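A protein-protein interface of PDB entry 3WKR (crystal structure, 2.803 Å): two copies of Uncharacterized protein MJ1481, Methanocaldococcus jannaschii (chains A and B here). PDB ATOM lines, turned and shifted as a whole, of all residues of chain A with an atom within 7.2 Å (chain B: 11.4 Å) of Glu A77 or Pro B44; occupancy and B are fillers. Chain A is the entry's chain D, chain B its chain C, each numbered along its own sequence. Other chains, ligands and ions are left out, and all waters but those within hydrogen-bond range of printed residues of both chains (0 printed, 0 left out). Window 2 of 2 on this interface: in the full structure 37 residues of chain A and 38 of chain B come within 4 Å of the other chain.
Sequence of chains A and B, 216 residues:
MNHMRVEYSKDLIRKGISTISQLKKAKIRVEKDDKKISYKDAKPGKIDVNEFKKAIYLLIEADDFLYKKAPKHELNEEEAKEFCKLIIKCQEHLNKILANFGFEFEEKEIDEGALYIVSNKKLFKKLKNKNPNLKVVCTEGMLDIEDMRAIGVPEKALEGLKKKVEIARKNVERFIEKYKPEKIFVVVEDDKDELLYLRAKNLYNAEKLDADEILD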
ATOM      1  N   GLU A  74       8.717  14.665  12.368  1.00  0.00           N
ATOM      2  CA  GLU A  74       8.391  13.246  12.314  1.00  0.00           C
ATOM      3  C   GLU A  74       9.159  12.459  13.369  1.00  0.00           C
ATOM      4  O   GLU A  74      10.390  12.465  13.390  1.00  0.00           O
ATOM      5  CB  GLU A  74       8.672  12.680  10.921  1.00  0.00           C
ATOM      6  CG  GLU A  74       7.795  13.265   9.828  1.00  0.00           C
ATOM      7  CD  GLU A  74       8.048  12.631   8.476  1.00  0.00           C
ATOM      8  OE1 GLU A  74       8.961  11.784   8.375  1.00  0.00           O
ATOM      9  OE2 GLU A  74       7.334  12.978   7.512  1.00  0.00           O
ATOM     10  N   LEU A  75       8.422  11.786  14.246  1.00  0.00           N
ATOM     11  CA  LEU A  75       9.026  11.001  15.312  1.00  0.00           C
ATOM     12  C   LEU A  75       9.048   9.524  14.943  1.00  0.00           C
ATOM     13  O   LEU A  75       8.184   9.048  14.206  1.00  0.00           O
ATOM     14  CB  LEU A  75       8.244  11.180  16.615  1.00  0.00           C
ATOM     15  CG  LEU A  75       7.879  12.601  17.052  1.00  0.00           C
ATOM     16  CD1 LEU A  75       7.157  12.568  18.389  1.00  0.00           C
ATOM     17  CD2 LEU A  75       9.108  13.487  17.129  1.00  0.00           C
ATOM     18  N   ASN A  76      10.039   8.800  15.453  1.00  0.00           N
ATOM     19  CA  ASN A  76      10.061   7.349  15.307  1.00  0.00           C
ATOM     20  C   ASN A  76       9.209   6.703  16.393  1.00  0.00           C
ATOM     21  O   ASN A  76       8.343   7.353  16.976  1.00  0.00           O
ATOM     22  CB  ASN A  76      11.495   6.808  15.327  1.00  0.00           C
ATOM     23  CG  ASN A  76      12.288   7.278  16.535  1.00  0.00           C
ATOM     24  OD1 ASN A  76      11.758   7.400  17.638  1.00  0.00           O
ATOM     25  ND2 ASN A  76      13.572   7.544  16.327  1.00  0.00           N
ATOM     26  N   GLU A  77       9.451   5.427  16.669  1.00  0.00           N
ATOM     27  CA  GLU A  77       8.689   4.735  17.702  1.00  0.00           C
ATOM     28  C   GLU A  77       9.171   5.132  19.092  1.00  0.00           C
ATOM     29  O   GLU A  77       8.381   5.225  20.031  1.00  0.00           O
ATOM     30  CB  GLU A  77       8.774   3.219  17.517  1.00  0.00           C
ATOM     31  CG  GLU A  77       7.900   2.419  18.475  1.00  0.00           C
ATOM     32  CD  GLU A  77       8.672   1.875  19.661  1.00  0.00           C
ATOM     33  OE1 GLU A  77       9.896   2.112  19.740  1.00  0.00           O
ATOM     34  OE2 GLU A  77       8.055   1.202  20.514  1.00  0.00           O
ATOM     35  N   GLU A  78      10.472   5.373  19.217  1.00  0.00           N
ATOM     36  CA  GLU A  78      11.060   5.718  20.505  1.00  0.00           C
ATOM     37  C   GLU A  78      10.782   7.174  20.868  1.00  0.00           C
ATOM     38  O   GLU A  78      10.570   7.501  22.036  1.00  0.00           O
ATOM     39  CB  GLU A  78      12.566   5.448  20.497  1.00  0.00           C
ATOM     40  CG  GLU A  78      13.195   5.388  21.881  1.00  0.00           C
ATOM     41  CD  GLU A  78      12.754   4.170  22.674  1.00  0.00           C
ATOM     42  OE1 GLU A  78      12.284   3.190  22.055  1.00  0.00           O
ATOM     43  OE2 GLU A  78      12.876   4.192  23.916  1.00  0.00           O
ATOM     44  N   GLU A  79      10.784   8.045  19.863  1.00  0.00           N
ATOM     45  CA  GLU A  79      10.510   9.461  20.079  1.00  0.00           C
ATOM     46  C   GLU A  79       9.025   9.709  20.330  1.00  0.00           C
ATOM     47  O   GLU A  79       8.653  10.678  20.992  1.00  0.00           O
ATOM     48  CB  GLU A  79      10.990  10.291  18.887  1.00  0.00           C
ATOM     49  CG  GLU A  79      12.502  10.343  18.737  1.00  0.00           C
ATOM     50  CD  GLU A  79      12.936  11.017  17.452  1.00  0.00           C
ATOM     51  OE1 GLU A  79      12.098  11.146  16.535  1.00  0.00           O
ATOM     52  OE2 GLU A  79      14.114  11.421  17.358  1.00  0.00           O
ATOM     53  N   ALA A  80       8.182   8.830  19.797  1.00  0.00           N
ATOM     54  CA  ALA A  80       6.742   8.936  20.001  1.00  0.00           C
ATOM     55  C   ALA A  80       6.372   8.560  21.430  1.00  0.00           C
ATOM     56  O   ALA A  80       5.550   9.224  22.062  1.00  0.00           O
ATOM     57  CB  ALA A  80       5.995   8.058  19.010  1.00  0.00           C
ATOM     58  N   LYS A  81       6.988   7.494  21.933  1.00  0.00           N
ATOM     59  CA  LYS A  81       6.743   7.032  23.295  1.00  0.00           C
ATOM     60  C   LYS A  81       7.117   8.097  24.318  1.00  0.00           C
ATOM     61  O   LYS A  81       6.420   8.284  25.313  1.00  0.00           O
ATOM     62  CB  LYS A  81       7.526   5.748  23.574  1.00  0.00           C
ATOM     63  CG  LYS A  81       7.022   4.535  22.814  1.00  0.00           C
ATOM     64  CD  LYS A  81       7.990   3.369  22.936  1.00  0.00           C
ATOM     65  CE  LYS A  81       8.180   2.952  24.384  1.00  0.00           C
ATOM     66  NZ  LYS A  81       9.174   1.850  24.513  1.00  0.00           N
ATOM     67  N   GLU A  82       8.221   8.791  24.064  1.00  0.00           N
ATOM     68  CA  GLU A  82       8.678   9.852  24.950  1.00  0.00           C
ATOM     69  C   GLU A  82       7.750  11.062  24.882  1.00  0.00           C
ATOM     70  O   GLU A  82       7.435  11.673  25.903  1.00  0.00           O
ATOM     71  CB  GLU A  82      10.107  10.267  24.590  1.00  0.00           C
ATOM     72  CG  GLU A  82      10.667  11.382  25.457  1.00  0.00           C
ATOM     73  CD  GLU A  82      12.044  11.831  25.010  1.00  0.00           C
ATOM     74  OE1 GLU A  82      12.530  11.326  23.977  1.00  0.00           O
ATOM     75  OE2 GLU A  82      12.640  12.690  25.693  1.00  0.00           O
ATOM     76  N   SER B  38      -1.887   3.556  26.800  1.00  0.00           N
ATOM     77  CA  SER B  38      -0.516   3.543  27.292  1.00  0.00           C
ATOM     78  C   SER B  38       0.412   4.271  26.326  1.00  0.00           C
ATOM     79  O   SER B  38       0.191   4.263  25.115  1.00  0.00           O
ATOM     80  CB  SER B  38      -0.035   2.106  27.504  1.00  0.00           C
ATOM     81  OG  SER B  38       1.295   2.079  27.993  1.00  0.00           O
ATOM     82  N   TYR B  39       1.451   4.897  26.866  1.00  0.00           N
ATOM     83  CA  TYR B  39       2.401   5.645  26.050  1.00  0.00           C
ATOM     84  C   TYR B  39       3.375   4.710  25.341  1.00  0.00           C
ATOM     85  O   TYR B  39       4.094   5.122  24.431  1.00  0.00           O
ATOM     86  CB  TYR B  39       3.173   6.652  26.906  1.00  0.00           C
ATOM     87  CG  TYR B  39       4.224   6.026  27.798  1.00  0.00           C
ATOM     88  CD1 TYR B  39       3.882   5.477  29.027  1.00  0.00           C
ATOM     89  CD2 TYR B  39       5.559   5.992  27.414  1.00  0.00           C
ATOM     90  CE1 TYR B  39       4.839   4.907  29.846  1.00  0.00           C
ATOM     91  CE2 TYR B  39       6.522   5.424  28.225  1.00  0.00           C
ATOM     92  CZ  TYR B  39       6.157   4.884  29.440  1.00  0.00           C
ATOM     93  OH  TYR B  39       7.113   4.319  30.253  1.00  0.00           O
ATOM     94  N   LYS B  40       3.398   3.453  25.767  1.00  0.00           N
ATOM     95  CA  LYS B  40       4.299   2.464  25.187  1.00  0.00           C
ATOM     96  C   LYS B  40       3.748   1.932  23.869  1.00  0.00           C
ATOM     97  O   LYS B  40       4.472   1.318  23.085  1.00  0.00           O
ATOM     98  CB  LYS B  40       4.535   1.318  26.170  1.00  0.00           C
ATOM     99  CG  LYS B  40       5.070   1.774  27.518  1.00  0.00           C
ATOM    100  CD  LYS B  40       5.209   0.613  28.486  1.00  0.00           C
ATOM    101  CE  LYS B  40       5.690   1.092  29.847  1.00  0.00           C
ATOM    102  NZ  LYS B  40       5.818  -0.028  30.819  1.00  0.00           N
ATOM    103  N   ASP B  41       2.463   2.176  23.632  1.00  0.00           N
ATOM    104  CA  ASP B  41       1.815   1.758  22.396  1.00  0.00           C
ATOM    105  C   ASP B  41       2.010   2.808  21.309  1.00  0.00           C
ATOM    106  O   ASP B  41       1.500   2.665  20.197  1.00  0.00           O
ATOM    107  CB  ASP B  41       0.321   1.527  22.629  1.00  0.00           C
ATOM    108  CG  ASP B  41       0.050   0.539  23.746  1.00  0.00           C
ATOM    109  OD1 ASP B  41       0.860  -0.394  23.927  1.00  0.00           O
ATOM    110  OD2 ASP B  41      -0.972   0.698  24.444  1.00  0.00           O
ATOM    111  N   ALA B  42       2.748   3.864  21.640  1.00  0.00           N
ATOM    112  CA  ALA B  42       2.973   4.966  20.712  1.00  0.00           C
ATOM    113  C   ALA B  42       3.744   4.520  19.476  1.00  0.00           C
ATOM    114  O   ALA B  42       4.876   4.045  19.568  1.00  0.00           O
ATOM    115  CB  ALA B  42       3.692   6.111  21.405  1.00  0.00           C
ATOM    116  N   LYS B  43       3.111   4.679  18.319  1.00  0.00           N
ATOM    117  CA  LYS B  43       3.715   4.319  17.046  1.00  0.00           C
ATOM    118  C   LYS B  43       4.180   5.583  16.324  1.00  0.00           C
ATOM    119  O   LYS B  43       3.621   6.658  16.541  1.00  0.00           O
ATOM    120  CB  LYS B  43       2.711   3.529  16.200  1.00  0.00           C
ATOM    121  CG  LYS B  43       2.368   2.166  16.785  1.00  0.00           C
ATOM    122  CD  LYS B  43       1.236   1.494  16.029  1.00  0.00           C
ATOM    123  CE  LYS B  43      -0.061   2.267  16.183  1.00  0.00           C
ATOM    124  NZ  LYS B  43      -1.186   1.619  15.455  1.00  0.00           N
ATOM    125  N   PRO B  44       5.221   5.461  15.481  1.00  0.00           N
ATOM    126  CA  PRO B  44       5.820   6.584  14.749  1.00  0.00           C
ATOM    127  C   PRO B  44       4.793   7.466  14.041  1.00  0.00           C
ATOM    128  O   PRO B  44       3.975   6.967  13.268  1.00  0.00           O
ATOM    129  CB  PRO B  44       6.702   5.885  13.714  1.00  0.00           C
ATOM    130  CG  PRO B  44       7.112   4.629  14.379  1.00  0.00           C
ATOM    131  CD  PRO B  44       5.940   4.199  15.223  1.00  0.00           C
ATOM    132  N   GLY B  45       4.845   8.767  14.309  1.00  0.00           N
ATOM    133  CA  GLY B  45       3.927   9.713  13.703  1.00  0.00           C
ATOM    134  C   GLY B  45       4.478  11.125  13.688  1.00  0.00           C
ATOM    135  O   GLY B  45       5.561  11.386  14.212  1.00  0.00           O
ATOM    136  N   LYS B  46       3.725  12.041  13.088  1.00  0.00           N
ATOM    137  CA  LYS B  46       4.149  13.431  12.977  1.00  0.00           C
ATOM    138  C   LYS B  46       3.441  14.319  13.996  1.00  0.00           C
ATOM    139  O   LYS B  46       2.242  14.171  14.235  1.00  0.00           O
ATOM    140  CB  LYS B  46       3.893  13.954  11.561  1.00  0.00           C
ATOM    141  CG  LYS B  46       4.277  15.409  11.353  1.00  0.00           C
ATOM    142  CD  LYS B  46       3.909  15.885   9.958  1.00  0.00           C
ATOM    143  CE  LYS B  46       4.233  17.358   9.778  1.00  0.00           C
ATOM    144  NZ  LYS B  46       3.500  18.210  10.756  1.00  0.00           N
ATOM    145  N   ILE B  47       4.191  15.239  14.594  1.00  0.00           N
ATOM    146  CA  ILE B  47       3.632  16.189  15.548  1.00  0.00           C
ATOM    147  C   ILE B  47       2.896  17.314  14.826  1.00  0.00           C
ATOM    148  O   ILE B  47       3.445  17.951  13.927  1.00  0.00           O
ATOM    149  CB  ILE B  47       4.729  16.803  16.439  1.00  0.00           C
ATOM    150  CG1 ILE B  47       5.452  15.710  17.229  1.00  0.00           C
ATOM    151  CG2 ILE B  47       4.136  17.841  17.381  1.00  0.00           C
ATOM    152  CD1 ILE B  47       6.540  16.235  18.138  1.00  0.00           C
ATOM    153  N   ASP B  48       1.649  17.551  15.223  1.00  0.00           N
ATOM    154  CA  ASP B  48       0.851  18.624  14.642  1.00  0.00           C
ATOM    155  C   ASP B  48       1.182  19.946  15.328  1.00  0.00           C
ATOM    156  O   ASP B  48       0.750  20.197  16.453  1.00  0.00           O
ATOM    157  CB  ASP B  48      -0.641  18.312  14.778  1.00  0.00           C
ATOM    158  CG  ASP B  48      -1.500  19.120  13.821  1.00  0.00           C
ATOM    159  OD1 ASP B  48      -1.136  20.273  13.507  1.00  0.00           O
ATOM    160  OD2 ASP B  48      -2.546  18.598  13.381  1.00  0.00           O
ATOM    161  N   ILE B  97      -3.586  15.195  18.871  1.00  0.00           N
ATOM    162  CA  ILE B  97      -2.139  15.068  18.760  1.00  0.00           C
ATOM    163  C   ILE B  97      -1.742  13.601  18.893  1.00  0.00           C
ATOM    164  O   ILE B  97      -0.888  13.107  18.155  1.00  0.00           O
ATOM    165  CB  ILE B  97      -1.412  15.907  19.831  1.00  0.00           C
ATOM    166  CG1 ILE B  97      -1.670  17.398  19.606  1.00  0.00           C
ATOM    167  CG2 ILE B  97       0.083  15.625  19.813  1.00  0.00           C
ATOM    168  CD1 ILE B  97      -0.995  18.297  20.619  1.00  0.00           C
ATOM    169  N   LEU B  98      -2.380  12.906  19.829  1.00  0.00           N
ATOM    170  CA  LEU B  98      -2.121  11.486  20.043  1.00  0.00           C
ATOM    171  C   LEU B  98      -2.636  10.640  18.881  1.00  0.00           C
ATOM    172  O   LEU B  98      -2.163   9.526  18.658  1.00  0.00           O
ATOM    173  CB  LEU B  98      -2.761  11.014  21.352  1.00  0.00           C
ATOM    174  CG  LEU B  98      -2.206  11.614  22.645  1.00  0.00           C
ATOM    175  CD1 LEU B  98      -2.964  11.081  23.851  1.00  0.00           C
ATOM    176  CD2 LEU B  98      -0.718  11.326  22.773  1.00  0.00           C
ATOM    177  N   ALA B  99      -3.598  11.180  18.139  1.00  0.00           N
ATOM    178  CA  ALA B  99      -4.212  10.463  17.025  1.00  0.00           C
ATOM    179  C   ALA B  99      -3.230  10.192  15.887  1.00  0.00           C
ATOM    180  O   ALA B  99      -3.486   9.356  15.020  1.00  0.00           O
ATOM    181  CB  ALA B  99      -5.427  11.224  16.510  1.00  0.00           C
ATOM    182  N   ASN B 100      -2.108  10.906  15.891  1.00  0.00           N
ATOM    183  CA  ASN B 100      -1.081  10.722  14.874  1.00  0.00           C
ATOM    184  C   ASN B 100      -0.065   9.653  15.265  1.00  0.00           C
ATOM    185  O   ASN B 100       0.773   9.256  14.456  1.00  0.00           O
ATOM    186  CB  ASN B 100      -0.364  12.044  14.591  1.00  0.00           C
ATOM    187  CG  ASN B 100      -1.293  13.101  14.029  1.00  0.00           C
ATOM    188  OD1 ASN B 100      -2.231  12.793  13.294  1.00  0.00           O
ATOM    189  ND2 ASN B 100      -1.037  14.357  14.375  1.00  0.00           N
ATOM    190  N   PHE B 101      -0.147   9.190  16.508  1.00  0.00           N
ATOM    191  CA  PHE B 101       0.790   8.195  17.014  1.00  0.00           C
ATOM    192  C   PHE B 101       0.091   6.887  17.372  1.00  0.00           C
ATOM    193  O   PHE B 101       0.534   6.160  18.261  1.00  0.00           O
ATOM    194  CB  PHE B 101       1.546   8.739  18.227  1.00  0.00           C
ATOM    195  CG  PHE B 101       2.241  10.046  17.969  1.00  0.00           C
ATOM    196  CD1 PHE B 101       3.485  10.076  17.362  1.00  0.00           C
ATOM    197  CD2 PHE B 101       1.650  11.243  18.334  1.00  0.00           C
ATOM    198  CE1 PHE B 101       4.126  11.277  17.123  1.00  0.00           C
ATOM    199  CE2 PHE B 101       2.286  12.448  18.099  1.00  0.00           C
ATOM    200  CZ  PHE B 101       3.526  12.464  17.493  1.00  0.00           C
ATOM    201  N   GLY B 102      -1.003   6.596  16.676  1.00  0.00           N
ATOM    202  CA  GLY B 102      -1.725   5.354  16.877  1.00  0.00           C
ATOM    203  C   GLY B 102      -2.599   5.348  18.117  1.00  0.00           C
ATOM    204  O   GLY B 102      -2.536   4.424  18.926  1.00  0.00           O
ATOM    205  N   PHE B 103      -3.415   6.386  18.265  1.00  0.00           N
ATOM    206  CA  PHE B 103      -4.359   6.465  19.374  1.00  0.00           C
ATOM    207  C   PHE B 103      -5.747   6.851  18.881  1.00  0.00           C
ATOM    208  O   PHE B 103      -5.896   7.433  17.806  1.00  0.00           O
ATOM    209  CB  PHE B 103      -3.878   7.463  20.430  1.00  0.00           C
ATOM    210  CG  PHE B 103      -2.679   6.997  21.205  1.00  0.00           C
ATOM    211  CD1 PHE B 103      -2.832   6.207  22.331  1.00  0.00           C
ATOM    212  CD2 PHE B 103      -1.400   7.352  20.808  1.00  0.00           C
ATOM    213  CE1 PHE B 103      -1.730   5.777  23.047  1.00  0.00           C
ATOM    214  CE2 PHE B 103      -0.295   6.925  21.520  1.00  0.00           C
ATOM    215  CZ  PHE B 103      -0.461   6.137  22.641  1.00  0.00           C
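The backbone NH of Lys B40 lies close to the side-chain hydroxyl of Ser B38 (3.4 Å). The backbone NH (N) of Lys B43 is in hydrogen-bond range of the backbone carbonyl oxygen (O) of Phe B101, at 3.0 Å. The side-chain amide oxygen (OD1) of Asn A76 sits at hydrogen-bond distance from the backbone NH (N) of Glu A78 (2.9 Å). The backbone NH (N) of Glu A79 lies within hydrogen-bond range of the side-chain amide oxygen (OD1) of Asn A76 (2.5 Å).
Of chain B, only Ala B42 and Pro B44 come within 4 Å of Glu A77. Of chain A, only Leu A75, Asn A76 and Glu A77 come within 4 Å of Pro B44. No residue of chain B comes within 4 Å of Glu A78. Ala A80 touches three residues of chain B. Of the printed residues of chain B, Lys A81 touches Tyr B39 (3.2 Å), Lys B40 (3.99 Å) and Ala B42 (3.6 Å). Of the printed residues of chain A, Ile B47 touches Leu A75 (3.7 Å). Of the printed residues of chain B, Glu A74 touches Gly B45. Printed residues of chain A within 4 Å of Phe B101: Leu A75 (3.5 Å) and Ala A80 (3.6 Å). The nearest printed residue of chain B that does not touch Glu A74 is Lys B46 (4.3 Å).
The backbone carbonyl oxygen of Gly B45 is in hydrogen-bond range of the backbone NH of Leu A75 (2.9 Å).
Of the 18 printed residues of chain B, 8 touch a printed residue of chain A. Hydrophobic or aromatic side chains of chain B that line the printed part of chain A: Tyr B39, Ala B42, Pro B44, Ile B47 and Phe B101. Of the 9 printed residues of chain A, 6 touch a printed residue of chain B. Along chain A the printed residues that touch a printed residue of chain B span positions 74 to 81. Among the printed residues, 14 pairs touch across the chains. Among the printed residues, no Asp or Glu carboxylate lies within 4 Å of a Lys or Arg side-chain nitrogen of the other chain.
No position is printed for both chains.
Among the printed residues, pairs that only touch across the chains: Glu A74 with Gly B45 (3.8 Å), Leu A75 with Pro B44 (3.5 Å), Leu A75 with Ile B47 (3.7 Å), Leu A75 with Phe B101 (3.5 Å), Asn A76 with Pro B44 (3.5 Å), Glu A77 with Ala B42 (3.6 Å), Glu A77 with Pro B44 (3.4 Å), Ala A80 with Ala B42 (3.6 Å), Ala A80 with Lys B43 (3.7 Å), Ala A80 with Phe B101 (3.6 Å), Lys A81 with Tyr B39 (3.2 Å), Lys A81 with Lys B40 (3.99 Å) and Lys A81 with Ala B42 (3.6 Å).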
